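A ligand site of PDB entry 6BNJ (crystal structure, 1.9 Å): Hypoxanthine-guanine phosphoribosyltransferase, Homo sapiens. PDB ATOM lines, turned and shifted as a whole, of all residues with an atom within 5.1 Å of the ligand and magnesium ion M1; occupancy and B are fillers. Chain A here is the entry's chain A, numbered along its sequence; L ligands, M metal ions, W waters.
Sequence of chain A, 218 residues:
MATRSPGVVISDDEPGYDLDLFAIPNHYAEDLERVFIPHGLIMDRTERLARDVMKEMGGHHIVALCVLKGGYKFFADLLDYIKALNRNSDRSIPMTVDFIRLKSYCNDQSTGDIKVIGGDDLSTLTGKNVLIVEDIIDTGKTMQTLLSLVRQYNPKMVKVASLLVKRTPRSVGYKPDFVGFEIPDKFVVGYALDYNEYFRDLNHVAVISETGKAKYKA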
ATOM      1  N   VAL A  67      17.939  -6.331 -10.621  1.00  0.00           N
ATOM      2  CA  VAL A  67      19.264  -6.322 -11.261  1.00  0.00           C
ATOM      3  C   VAL A  67      19.174  -6.037 -12.783  1.00  0.00           C
ATOM      4  O   VAL A  67      18.778  -6.885 -13.622  1.00  0.00           O
ATOM      5  CB  VAL A  67      20.030  -7.626 -10.980  1.00  0.00           C
ATOM      6  CG1 VAL A  67      21.496  -7.509 -11.479  1.00  0.00           C
ATOM      7  CG2 VAL A  67      19.956  -7.971  -9.459  1.00  0.00           C
ATOM      8  N   LEU A  68      19.533  -4.809 -13.144  1.00  0.00           N
ATOM      9  CA  LEU A  68      19.469  -4.325 -14.551  1.00  0.00           C
ATOM     10  C   LEU A  68      20.637  -4.868 -15.365  1.00  0.00           C
ATOM     11  O   LEU A  68      21.689  -5.142 -14.787  1.00  0.00           O
ATOM     12  CB  LEU A  68      19.476  -2.784 -14.584  1.00  0.00           C
ATOM     13  CG  LEU A  68      18.223  -2.132 -13.994  1.00  0.00           C
ATOM     14  CD1 LEU A  68      18.400  -0.651 -13.809  1.00  0.00           C
ATOM     15  CD2 LEU A  68      16.976  -2.483 -14.848  1.00  0.00           C
ATOM     16  N   LYS A  69      20.484  -4.970 -16.695  1.00  0.00           N
ATOM     17  CA  LYS A  69      19.245  -4.633 -17.401  1.00  0.00           C
ATOM     18  C   LYS A  69      18.309  -5.817 -17.474  1.00  0.00           C
ATOM     19  O   LYS A  69      17.087  -5.676 -17.544  1.00  0.00           O
ATOM     20  CB  LYS A  69      19.536  -4.180 -18.842  1.00  0.00           C
ATOM     21  CG  LYS A  69      20.280  -2.877 -18.975  1.00  0.00           C
ATOM     22  CD  LYS A  69      20.511  -2.607 -20.487  1.00  0.00           C
ATOM     23  CE  LYS A  69      21.357  -1.384 -20.770  1.00  0.00           C
ATOM     24  NZ  LYS A  69      21.585  -1.342 -22.256  1.00  0.00           N
ATOM     25  N   GLY A  70      18.912  -6.990 -17.547  1.00  0.00           N
ATOM     26  CA  GLY A  70      18.214  -8.203 -17.832  1.00  0.00           C
ATOM     27  C   GLY A  70      17.088  -8.572 -16.875  1.00  0.00           C
ATOM     28  O   GLY A  70      16.191  -9.253 -17.279  1.00  0.00           O
ATOM     29  N   GLY A  71      17.157  -8.185 -15.613  1.00  0.00           N
ATOM     30  CA  GLY A  71      16.032  -8.556 -14.719  1.00  0.00           C
ATOM     31  C   GLY A  71      14.779  -7.701 -14.875  1.00  0.00           C
ATOM     32  O   GLY A  71      13.755  -7.979 -14.199  1.00  0.00           O
ATOM     33  N   ARG A 101      22.823  -2.012 -11.177  1.00  0.00           N
ATOM     34  CA  ARG A 101      23.283  -2.547 -12.444  1.00  0.00           C
ATOM     35  C   ARG A 101      24.631  -3.143 -12.245  1.00  0.00           C
ATOM     36  O   ARG A 101      25.475  -2.542 -11.573  1.00  0.00           O
ATOM     37  CB  ARG A 101      23.332  -1.467 -13.522  1.00  0.00           C
ATOM     38  CG  ARG A 101      24.174  -1.908 -14.709  1.00  0.00           C
ATOM     39  CD  ARG A 101      23.349  -2.026 -15.958  1.00  0.00           C
ATOM     40  NE  ARG A 101      23.364  -0.811 -16.748  1.00  0.00           N
ATOM     41  CZ  ARG A 101      23.979  -0.679 -17.918  1.00  0.00           C
ATOM     42  NH1 ARG A 101      24.633  -1.689 -18.481  1.00  0.00           N
ATOM     43  NH2 ARG A 101      23.911   0.488 -18.541  1.00  0.00           N
ATOM     44  N   LEU A 102      24.825  -4.357 -12.763  1.00  0.00           N
ATOM     45  CA  LEU A 102      26.119  -5.041 -12.704  1.00  0.00           C
ATOM     46  C   LEU A 102      26.659  -5.168 -14.112  1.00  0.00           C
ATOM     47  O   LEU A 102      25.931  -5.637 -15.002  1.00  0.00           O
ATOM     48  CB  LEU A 102      26.000  -6.408 -12.028  1.00  0.00           C
ATOM     49  CG  LEU A 102      25.482  -6.258 -10.587  1.00  0.00           C
ATOM     50  CD1 LEU A 102      25.568  -7.570  -9.832  1.00  0.00           C
ATOM     51  CD2 LEU A 102      26.226  -5.132  -9.841  1.00  0.00           C
ATOM     52  N   ASP A 135      17.464 -12.065 -13.943  1.00  0.00           N
ATOM     53  CA  ASP A 135      17.061 -12.836 -15.114  1.00  0.00           C
ATOM     54  C   ASP A 135      17.642 -14.272 -15.067  1.00  0.00           C
ATOM     55  O   ASP A 135      16.921 -15.223 -15.327  1.00  0.00           O
ATOM     56  CB  ASP A 135      17.464 -12.143 -16.424  1.00  0.00           C
ATOM     57  CG  ASP A 135      18.933 -11.730 -16.468  1.00  0.00           C
ATOM     58  OD1 ASP A 135      19.603 -11.761 -15.423  1.00  0.00           O
ATOM     59  OD2 ASP A 135      19.431 -11.404 -17.570  1.00  0.00           O
ATOM     60  N   ILE A 136      18.922 -14.428 -14.755  1.00  0.00           N
ATOM     61  CA  ILE A 136      19.527 -15.756 -14.874  1.00  0.00           C
ATOM     62  C   ILE A 136      20.750 -15.941 -13.956  1.00  0.00           C
ATOM     63  O   ILE A 136      21.563 -15.033 -13.799  1.00  0.00           O
ATOM     64  CB  ILE A 136      19.931 -16.074 -16.371  1.00  0.00           C
ATOM     65  CG1 ILE A 136      20.477 -17.501 -16.526  1.00  0.00           C
ATOM     66  CG2 ILE A 136      20.940 -15.077 -16.977  1.00  0.00           C
ATOM     67  CD1 ILE A 136      20.316 -17.958 -17.980  1.00  0.00           C
ATOM     68  N   ILE A 137      20.814 -17.121 -13.358  1.00  0.00           N
ATOM     69  CA  ILE A 137      21.973 -17.587 -12.636  1.00  0.00           C
ATOM     70  C   ILE A 137      22.679 -18.664 -13.471  1.00  0.00           C
ATOM     71  O   ILE A 137      22.075 -19.670 -13.872  1.00  0.00           O
ATOM     72  CB  ILE A 137      21.577 -18.072 -11.268  1.00  0.00           C
ATOM     73  CG1 ILE A 137      21.134 -16.829 -10.488  1.00  0.00           C
ATOM     74  CG2 ILE A 137      22.761 -18.753 -10.605  1.00  0.00           C
ATOM     75  CD1 ILE A 137      20.402 -17.106  -9.297  1.00  0.00           C
ATOM     76  N   ASP A 138      23.951 -18.410 -13.789  1.00  0.00           N
ATOM     77  CA  ASP A 138      24.758 -19.329 -14.585  1.00  0.00           C
ATOM     78  C   ASP A 138      25.818 -19.944 -13.664  1.00  0.00           C
ATOM     79  O   ASP A 138      25.575 -21.003 -13.086  1.00  0.00           O
ATOM     80  CB  ASP A 138      25.347 -18.587 -15.803  1.00  0.00           C
ATOM     81  CG  ASP A 138      26.188 -19.489 -16.702  1.00  0.00           C
ATOM     82  OD1 ASP A 138      26.066 -20.726 -16.604  1.00  0.00           O
ATOM     83  OD2 ASP A 138      26.984 -18.954 -17.498  1.00  0.00           O
ATOM     84  N   THR A 139      26.961 -19.283 -13.479  1.00  0.00           N
ATOM     85  CA  THR A 139      27.945 -19.760 -12.508  1.00  0.00           C
ATOM     86  C   THR A 139      27.506 -19.491 -11.052  1.00  0.00           C
ATOM     87  O   THR A 139      27.971 -20.163 -10.129  1.00  0.00           O
ATOM     88  CB  THR A 139      29.355 -19.112 -12.725  1.00  0.00           C
ATOM     89  OG1 THR A 139      29.326 -17.696 -12.428  1.00  0.00           O
ATOM     90  CG2 THR A 139      29.857 -19.355 -14.155  1.00  0.00           C
ATOM     91  N   GLY A 140      26.638 -18.514 -10.845  1.00  0.00           N
ATOM     92  CA  GLY A 140      26.304 -18.058  -9.505  1.00  0.00           C
ATOM     93  C   GLY A 140      27.328 -17.074  -8.901  1.00  0.00           C
ATOM     94  O   GLY A 140      27.118 -16.584  -7.791  1.00  0.00           O
ATOM     95  N   LYS A 141      28.425 -16.770  -9.601  1.00  0.00           N
ATOM     96  CA  LYS A 141      29.417 -15.872  -9.012  1.00  0.00           C
ATOM     97  C   LYS A 141      28.926 -14.446  -8.880  1.00  0.00           C
ATOM     98  O   LYS A 141      29.226 -13.772  -7.878  1.00  0.00           O
ATOM     99  CB  LYS A 141      30.722 -15.890  -9.812  1.00  0.00           C
ATOM    100  CG  LYS A 141      31.435 -17.203  -9.753  1.00  0.00           C
ATOM    101  CD  LYS A 141      32.735 -17.198 -10.573  1.00  0.00           C
ATOM    102  CE  LYS A 141      33.296 -18.602 -10.613  1.00  0.00           C
ATOM    103  NZ  LYS A 141      34.700 -18.666 -11.120  1.00  0.00           N
ATOM    104  N   THR A 142      28.179 -13.971  -9.868  1.00  0.00           N
ATOM    105  CA  THR A 142      27.613 -12.606  -9.814  1.00  0.00           C
ATOM    106  C   THR A 142      26.733 -12.462  -8.593  1.00  0.00           C
ATOM    107  O   THR A 142      26.843 -11.497  -7.832  1.00  0.00           O
ATOM    108  CB  THR A 142      26.773 -12.267 -11.080  1.00  0.00           C
ATOM    109  OG1 THR A 142      27.634 -12.286 -12.212  1.00  0.00           O
ATOM    110  CG2 THR A 142      26.085 -10.905 -10.983  1.00  0.00           C
ATOM    111  N   MET A 143      25.848 -13.446  -8.392  1.00  0.00           N
ATOM    112  CA  MET A 143      24.945 -13.380  -7.255  1.00  0.00           C
ATOM    113  C   MET A 143      25.668 -13.510  -5.931  1.00  0.00           C
ATOM    114  O   MET A 143      25.300 -12.839  -4.984  1.00  0.00           O
ATOM    115  CB  MET A 143      23.843 -14.448  -7.333  1.00  0.00           C
ATOM    116  CG  MET A 143      22.757 -14.202  -6.314  1.00  0.00           C
ATOM    117  SD  MET A 143      22.084 -12.510  -6.372  1.00  0.00           S
ATOM    118  CE  MET A 143      21.496 -12.451  -8.025  1.00  0.00           C
ATOM    119  N   LYS A 166      20.729 -22.067 -14.902  1.00  0.00           N
ATOM    120  CA  LYS A 166      21.320 -23.072 -15.774  1.00  0.00           C
ATOM    121  C   LYS A 166      21.848 -24.271 -14.990  1.00  0.00           C
ATOM    122  O   LYS A 166      22.421 -24.118 -13.885  1.00  0.00           O
ATOM    123  CB  LYS A 166      22.458 -22.479 -16.595  1.00  0.00           C
ATOM    124  CG  LYS A 166      21.998 -21.650 -17.716  1.00  0.00           C
ATOM    125  CD  LYS A 166      23.171 -21.294 -18.649  1.00  0.00           C
ATOM    126  CE  LYS A 166      22.632 -20.556 -19.865  1.00  0.00           C
ATOM    127  NZ  LYS A 166      23.703 -19.877 -20.673  1.00  0.00           N
ATOM    128  N   LYS A 186      22.697 -23.718 -22.369  1.00  0.00           N
ATOM    129  CA  LYS A 186      22.443 -23.186 -23.725  1.00  0.00           C
ATOM    130  C   LYS A 186      22.265 -21.677 -23.634  1.00  0.00           C
ATOM    131  O   LYS A 186      21.686 -21.194 -22.661  1.00  0.00           O
ATOM    132  CB  LYS A 186      21.148 -23.743 -24.340  1.00  0.00           C
ATOM    133  CG  LYS A 186      21.200 -25.130 -24.923  1.00  0.00           C
ATOM    134  CD  LYS A 186      19.819 -25.465 -25.467  1.00  0.00           C
ATOM    135  CE  LYS A 186      19.778 -26.890 -26.024  1.00  0.00           C
ATOM    136  NZ  LYS A 186      18.349 -27.349 -26.188  1.00  0.00           N
ATOM    137  N   PHE A 187      22.651 -20.938 -24.675  1.00  0.00           N
ATOM    138  CA  PHE A 187      22.493 -19.497 -24.664  1.00  0.00           C
ATOM    139  C   PHE A 187      21.082 -19.106 -25.099  1.00  0.00           C
ATOM    140  O   PHE A 187      20.643 -19.455 -26.191  1.00  0.00           O
ATOM    141  CB  PHE A 187      23.515 -18.851 -25.569  1.00  0.00           C
ATOM    142  CG  PHE A 187      23.566 -17.345 -25.412  1.00  0.00           C
ATOM    143  CD1 PHE A 187      24.188 -16.766 -24.316  1.00  0.00           C
ATOM    144  CD2 PHE A 187      22.941 -16.528 -26.334  1.00  0.00           C
ATOM    145  CE1 PHE A 187      24.204 -15.394 -24.139  1.00  0.00           C
ATOM    146  CE2 PHE A 187      22.955 -15.158 -26.148  1.00  0.00           C
ATOM    147  CZ  PHE A 187      23.562 -14.603 -25.061  1.00  0.00           C
ATOM    148  N   VAL A 188      20.353 -18.425 -24.219  1.00  0.00           N
ATOM    149  CA  VAL A 188      19.014 -18.040 -24.557  1.00  0.00           C
ATOM    150  C   VAL A 188      18.908 -16.525 -24.601  1.00  0.00           C
ATOM    151  O   VAL A 188      19.708 -15.805 -23.977  1.00  0.00           O
ATOM    152  CB  VAL A 188      18.002 -18.642 -23.555  1.00  0.00           C
ATOM    153  CG1 VAL A 188      18.081 -20.194 -23.665  1.00  0.00           C
ATOM    154  CG2 VAL A 188      18.311 -18.131 -22.160  1.00  0.00           C
ATOM    155  N   VAL A 189      17.908 -16.049 -25.342  1.00  0.00           N
ATOM    156  CA  VAL A 189      17.616 -14.617 -25.421  1.00  0.00           C
ATOM    157  C   VAL A 189      16.110 -14.380 -25.251  1.00  0.00           C
ATOM    158  O   VAL A 189      15.320 -15.319 -25.330  1.00  0.00           O
ATOM    159  CB  VAL A 189      18.052 -14.021 -26.789  1.00  0.00           C
ATOM    160  CG1 VAL A 189      19.557 -14.107 -26.934  1.00  0.00           C
ATOM    161  CG2 VAL A 189      17.354 -14.741 -27.976  1.00  0.00           C
ATOM    162  N   LEU A 193      16.511 -10.816 -21.775  1.00  0.00           N
ATOM    163  CA  LEU A 193      17.839 -11.442 -21.962  1.00  0.00           C
ATOM    164  C   LEU A 193      18.374 -11.084 -23.346  1.00  0.00           C
ATOM    165  O   LEU A 193      17.703 -11.332 -24.362  1.00  0.00           O
ATOM    166  CB  LEU A 193      17.756 -12.975 -21.792  1.00  0.00           C
ATOM    167  CG  LEU A 193      17.625 -13.281 -20.284  1.00  0.00           C
ATOM    168  CD1 LEU A 193      16.212 -13.521 -19.904  1.00  0.00           C
ATOM    169  CD2 LEU A 193      18.486 -14.480 -19.879  1.00  0.00           C
ATOM    170  N   ASP A 194      19.556 -10.511 -23.386  1.00  0.00           N
ATOM    171  CA  ASP A 194      20.045 -10.000 -24.644  1.00  0.00           C
ATOM    172  C   ASP A 194      21.194 -10.784 -25.237  1.00  0.00           C
ATOM    173  O   ASP A 194      21.903 -11.524 -24.563  1.00  0.00           O
ATOM    174  CB  ASP A 194      20.511  -8.547 -24.461  1.00  0.00           C
ATOM    175  CG  ASP A 194      21.842  -8.467 -23.709  1.00  0.00           C
ATOM    176  OD1 ASP A 194      21.910  -8.964 -22.571  1.00  0.00           O
ATOM    177  OD2 ASP A 194      22.803  -7.901 -24.263  1.00  0.00           O
ATOM    178  N   TYR A 195      21.441 -10.502 -26.507  1.00  0.00           N
ATOM    179  CA  TYR A 195      22.676 -10.816 -27.187  1.00  0.00           C
ATOM    180  C   TYR A 195      23.204  -9.508 -27.777  1.00  0.00           C
ATOM    181  O   TYR A 195      22.606  -8.955 -28.691  1.00  0.00           O
ATOM    182  CB  TYR A 195      22.421 -11.865 -28.279  1.00  0.00           C
ATOM    183  CG  TYR A 195      23.600 -12.227 -29.135  1.00  0.00           C
ATOM    184  CD1 TYR A 195      24.689 -12.917 -28.623  1.00  0.00           C
ATOM    185  CD2 TYR A 195      23.624 -11.865 -30.489  1.00  0.00           C
ATOM    186  CE1 TYR A 195      25.786 -13.264 -29.452  1.00  0.00           C
ATOM    187  CE2 TYR A 195      24.675 -12.223 -31.313  1.00  0.00           C
ATOM    188  CZ  TYR A 195      25.766 -12.921 -30.780  1.00  0.00           C
ATOM    189  OH  TYR A 195      26.819 -13.257 -31.601  1.00  0.00           O
ATOM    190  N   ARG A 200      16.097  -7.933 -26.348  1.00  0.00           N
ATOM    191  CA  ARG A 200      15.375  -7.583 -25.146  1.00  0.00           C
ATOM    192  C   ARG A 200      13.922  -7.254 -25.477  1.00  0.00           C
ATOM    193  O   ARG A 200      13.035  -7.437 -24.622  1.00  0.00           O
ATOM    194  CB  ARG A 200      16.025  -6.393 -24.389  1.00  0.00           C
ATOM    195  CG  ARG A 200      17.453  -6.677 -23.973  1.00  0.00           C
ATOM    196  CD  ARG A 200      17.865  -5.735 -22.814  1.00  0.00           C
ATOM    197  NE  ARG A 200      19.311  -5.574 -22.704  1.00  0.00           N
ATOM    198  CZ  ARG A 200      20.081  -6.274 -21.906  1.00  0.00           C
ATOM    199  NH1 ARG A 200      19.542  -7.229 -21.123  1.00  0.00           N
ATOM    200  NH2 ARG A 200      21.397  -6.019 -21.867  1.00  0.00           N
HETATM  201  C1  LIG L   1      23.255 -14.898 -20.170  1.00  0.00           C
HETATM  202  C2  LIG L   1      23.091 -16.264 -20.385  1.00  0.00           C
HETATM  203  C3  LIG L   1      22.209 -16.667 -21.433  1.00  0.00           C
HETATM  204  C4  LIG L   1      24.474 -16.038 -18.651  1.00  0.00           C
HETATM  205  N1  LIG L   1      21.606 -15.713 -22.197  1.00  0.00           N
HETATM  206  N2  LIG L   1      21.106 -13.431 -22.805  1.00  0.00           N
HETATM  207  N3  LIG L   1      22.608 -13.971 -20.985  1.00  0.00           N
HETATM  208  O1  LIG L   1      27.670 -14.792 -12.258  1.00  0.00           O
HETATM  209  P1  LIG L   1      26.744 -15.572 -13.276  1.00  0.00           P
HETATM  210  O2  LIG L   1      25.713 -16.495 -12.569  1.00  0.00           O
HETATM  211  O3  LIG L   1      27.589 -16.366 -14.241  1.00  0.00           O
HETATM  212  C5  LIG L   1      25.892 -14.263 -14.258  1.00  0.00           C
HETATM  213  O4  LIG L   1      26.892 -13.537 -14.880  1.00  0.00           O
HETATM  214  C6  LIG L   1      24.937 -14.838 -15.285  1.00  0.00           C
HETATM  215  O5  LIG L   1      24.402 -13.933 -16.226  1.00  0.00           O
HETATM  216  C7  LIG L   1      25.198 -13.479 -17.271  1.00  0.00           C
HETATM  217  C8  LIG L   1      25.401 -12.039 -17.052  1.00  0.00           C
HETATM  218  N4  LIG L   1      25.215 -11.435 -18.384  1.00  0.00           N
HETATM  219  C9  LIG L   1      24.960 -10.047 -18.702  1.00  0.00           C
HETATM  220  O6  LIG L   1      24.838  -9.712 -19.875  1.00  0.00           O
HETATM  221  C10 LIG L   1      24.889  -9.022 -17.608  1.00  0.00           C
HETATM  222  C11 LIG L   1      24.508  -7.645 -18.120  1.00  0.00           C
HETATM  223  P2  LIG L   1      22.712  -7.471 -18.497  1.00  0.00           P
HETATM  224  O7  LIG L   1      22.362  -8.124 -19.876  1.00  0.00           O
HETATM  225  O8  LIG L   1      22.465  -5.908 -18.539  1.00  0.00           O
HETATM  226  O9  LIG L   1      21.809  -8.063 -17.404  1.00  0.00           O
HETATM  227  C12 LIG L   1      25.281 -12.498 -19.401  1.00  0.00           C
HETATM  228  C13 LIG L   1      24.537 -13.488 -18.586  1.00  0.00           C
HETATM  229  N5  LIG L   1      24.137 -14.810 -19.098  1.00  0.00           N
HETATM  230  C14 LIG L   1      21.785 -14.395 -21.974  1.00  0.00           C
HETATM  231  O10 LIG L   1      21.993 -18.012 -21.684  1.00  0.00           O
HETATM  232  N6  LIG L   1      23.859 -16.976 -19.451  1.00  0.00           N
HETATM  233 MG    MG M   1      23.363  -9.404 -21.211  1.00  0.00          MG
HETATM  234 MG    MG M   2      21.469 -10.848 -14.716  1.00  0.00          MG
HETATM  235  O   HOH W   1      25.971 -10.812 -13.805  1.00  0.00           O
HETATM  236  O   HOH W   2      30.319 -14.464 -13.080  1.00  0.00           O
HETATM  237  O   HOH W   3      20.114 -10.055 -19.757  1.00  0.00           O
HETATM  238  O   HOH W   4      24.173 -10.889 -22.771  1.00  0.00           O
HETATM  239  O   HOH W   5      22.026 -10.644 -16.781  1.00  0.00           O
HETATM  240  O   HOH W   6      20.441  -8.755 -15.043  1.00  0.00           O
HETATM  241  O   HOH W   7      22.264 -11.166 -20.578  1.00  0.00           O
HETATM  242  O   HOH W   8      26.561 -15.109 -21.339  1.00  0.00           O
HETATM  243  O   HOH W   9      24.702 -15.215 -10.255  1.00  0.00           O
HETATM  244  O   HOH W  10      24.207  -4.968 -20.594  1.00  0.00           O
HETATM  245  O   HOH W  11      24.614  -7.907 -22.070  1.00  0.00           O
HETATM  246  O   HOH W  12      23.525  -7.415 -14.537  1.00  0.00           O
HETATM  247  O   HOH W  13      28.079 -16.362 -16.618  1.00  0.00           O
HETATM  248  O   HOH W  14      22.277 -12.740 -14.774  1.00  0.00           O
HETATM  249  O   HOH W  15      24.180  -4.413 -17.136  1.00  0.00           O
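The backbone carbonyl oxygen of Asp 194 is in hydrogen-bond range of a nitrogen (N2) of the ligand, at 2.7 Å.
N of Thr 142 sits at hydrogen-bond distance from O1 of the ligand (2.6 Å).
The side-chain hydroxyl (OG1) of Thr 142 sits at hydrogen-bond distance from an oxygen (O1) of the ligand, 2.5 Å away.
An oxygen (O10) of the ligand sits at hydrogen-bond distance from the backbone NH of Val 188, 3.0 Å away.
A nitrogen (N1) of the ligand sits at hydrogen-bond distance from the backbone carbonyl oxygen (O) of Val 188 (2.6 Å).
NZ of Lys 166 lies within hydrogen-bond range of O10 of the ligand (2.7 Å).
N of Gly 140 lies within hydrogen-bond range of O2 of the ligand, 2.8 Å away.
The backbone NH of Thr 139 is in hydrogen-bond range of an oxygen (O3) of the ligand, at 3.1 Å.
O3 of the ligand sits at hydrogen-bond distance from OG1 of Thr 139 (2.8 Å).
N of Lys 69 sits at hydrogen-bond distance from O8 of the ligand, at 2.9 Å.
The backbone NH (N) of Asp 138 sits at hydrogen-bond distance from an oxygen (O2) of the ligand (2.9 Å).
NH2 of Arg 200 is in salt-bridge range of O8 of the ligand, at 3.5 Å.
O9 of the ligand lies within hydrogen-bond range of N of Gly 70 (3.1 Å).
O1 of the ligand sits at hydrogen-bond distance from N of Lys 141 (3.4 Å).
The guanidinium group of Arg 200 lies within salt-bridge range of the side-chain carboxylate of Asp 194 (3.4 Å).
O of Lys 186 sits close to NZ of Lys 166, 3.1 Å away.
The backbone NH (N) of Lys 166 sits at hydrogen-bond distance from the backbone carbonyl oxygen (O) of Ile 137 (2.9 Å).
The side-chain hydroxyl (OG1) of Thr 139 lies within hydrogen-bond range of the backbone NH (N) of Lys 141 (3.1 Å).
O of Lys 186 lies close to O10 of the ligand, at 3.3 Å.
Leu 68 touches the ligand.
Leu 102 touches the ligand.
Ile 136 touches the ligand (O to C6, 3.7 Å).
Ile 137 touches the ligand (C to O2, 3.8 Å).
CE1 of Phe 187 touches N1 of the ligand, at 3.3 Å.
Leu 193 touches the ligand (CB to N2, 3.5 Å).
18 residues have an atom within 4 Å of the ligand: Leu 68, Lys 69, Gly 70, Leu 102, Ile 136, Ile 137, Asp 138, Thr 139, Gly 140, Lys 141, Thr 142, Lys 166, Lys 186, Phe 187, Val 188, Leu 193, Asp 194 and Arg 200.
Arg 200 touches magnesium ion M1 (NH2 to MG, 3.97 Å).
Within 4 Å of magnesium ion M1: Asp 194 and Arg 200.
The nearest printed residue that does not touch magnesium ion M1 is Leu 193 (5.7 Å).
An oxygen (O6) of the ligand is bound to magnesium ion M1, at 2.0 Å.
OD1 of Asp 194 binds magnesium ion M1, at 2.0 Å.
O7 of the ligand binds magnesium ion M1.
Water W11 is bound to magnesium ion M1, at 2.1 Å.
Magnesium ion M1 is bound by water W7 (2.2 Å).
Water W4 is bound to magnesium ion M1 (2.3 Å).
Water W5 lies within hydrogen-bond range of O9 of the ligand (2.7 Å) and OD2 of Asp 135 (2.8 Å).
Water W15 lies within hydrogen-bond range of O8 of the ligand, O of Leu 102 and NH1 of Arg 101.
Water W9 bridges the backbone NH of Met 143 and an oxygen (O2) of the ligand.
Water W14 lies within hydrogen-bond range of the backbone carbonyl oxygen (O) of Ile 136 (2.6 Å) and an oxygen (O5) of the ligand (2.8 Å).
Water W10 bridges O8 of the ligand (2.9 Å) and NH2 of Arg 200 (3.3 Å).
Water W1 lies within hydrogen-bond range of OG1 of Thr 142 (2.7 Å) and O4 of the ligand (3.1 Å).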
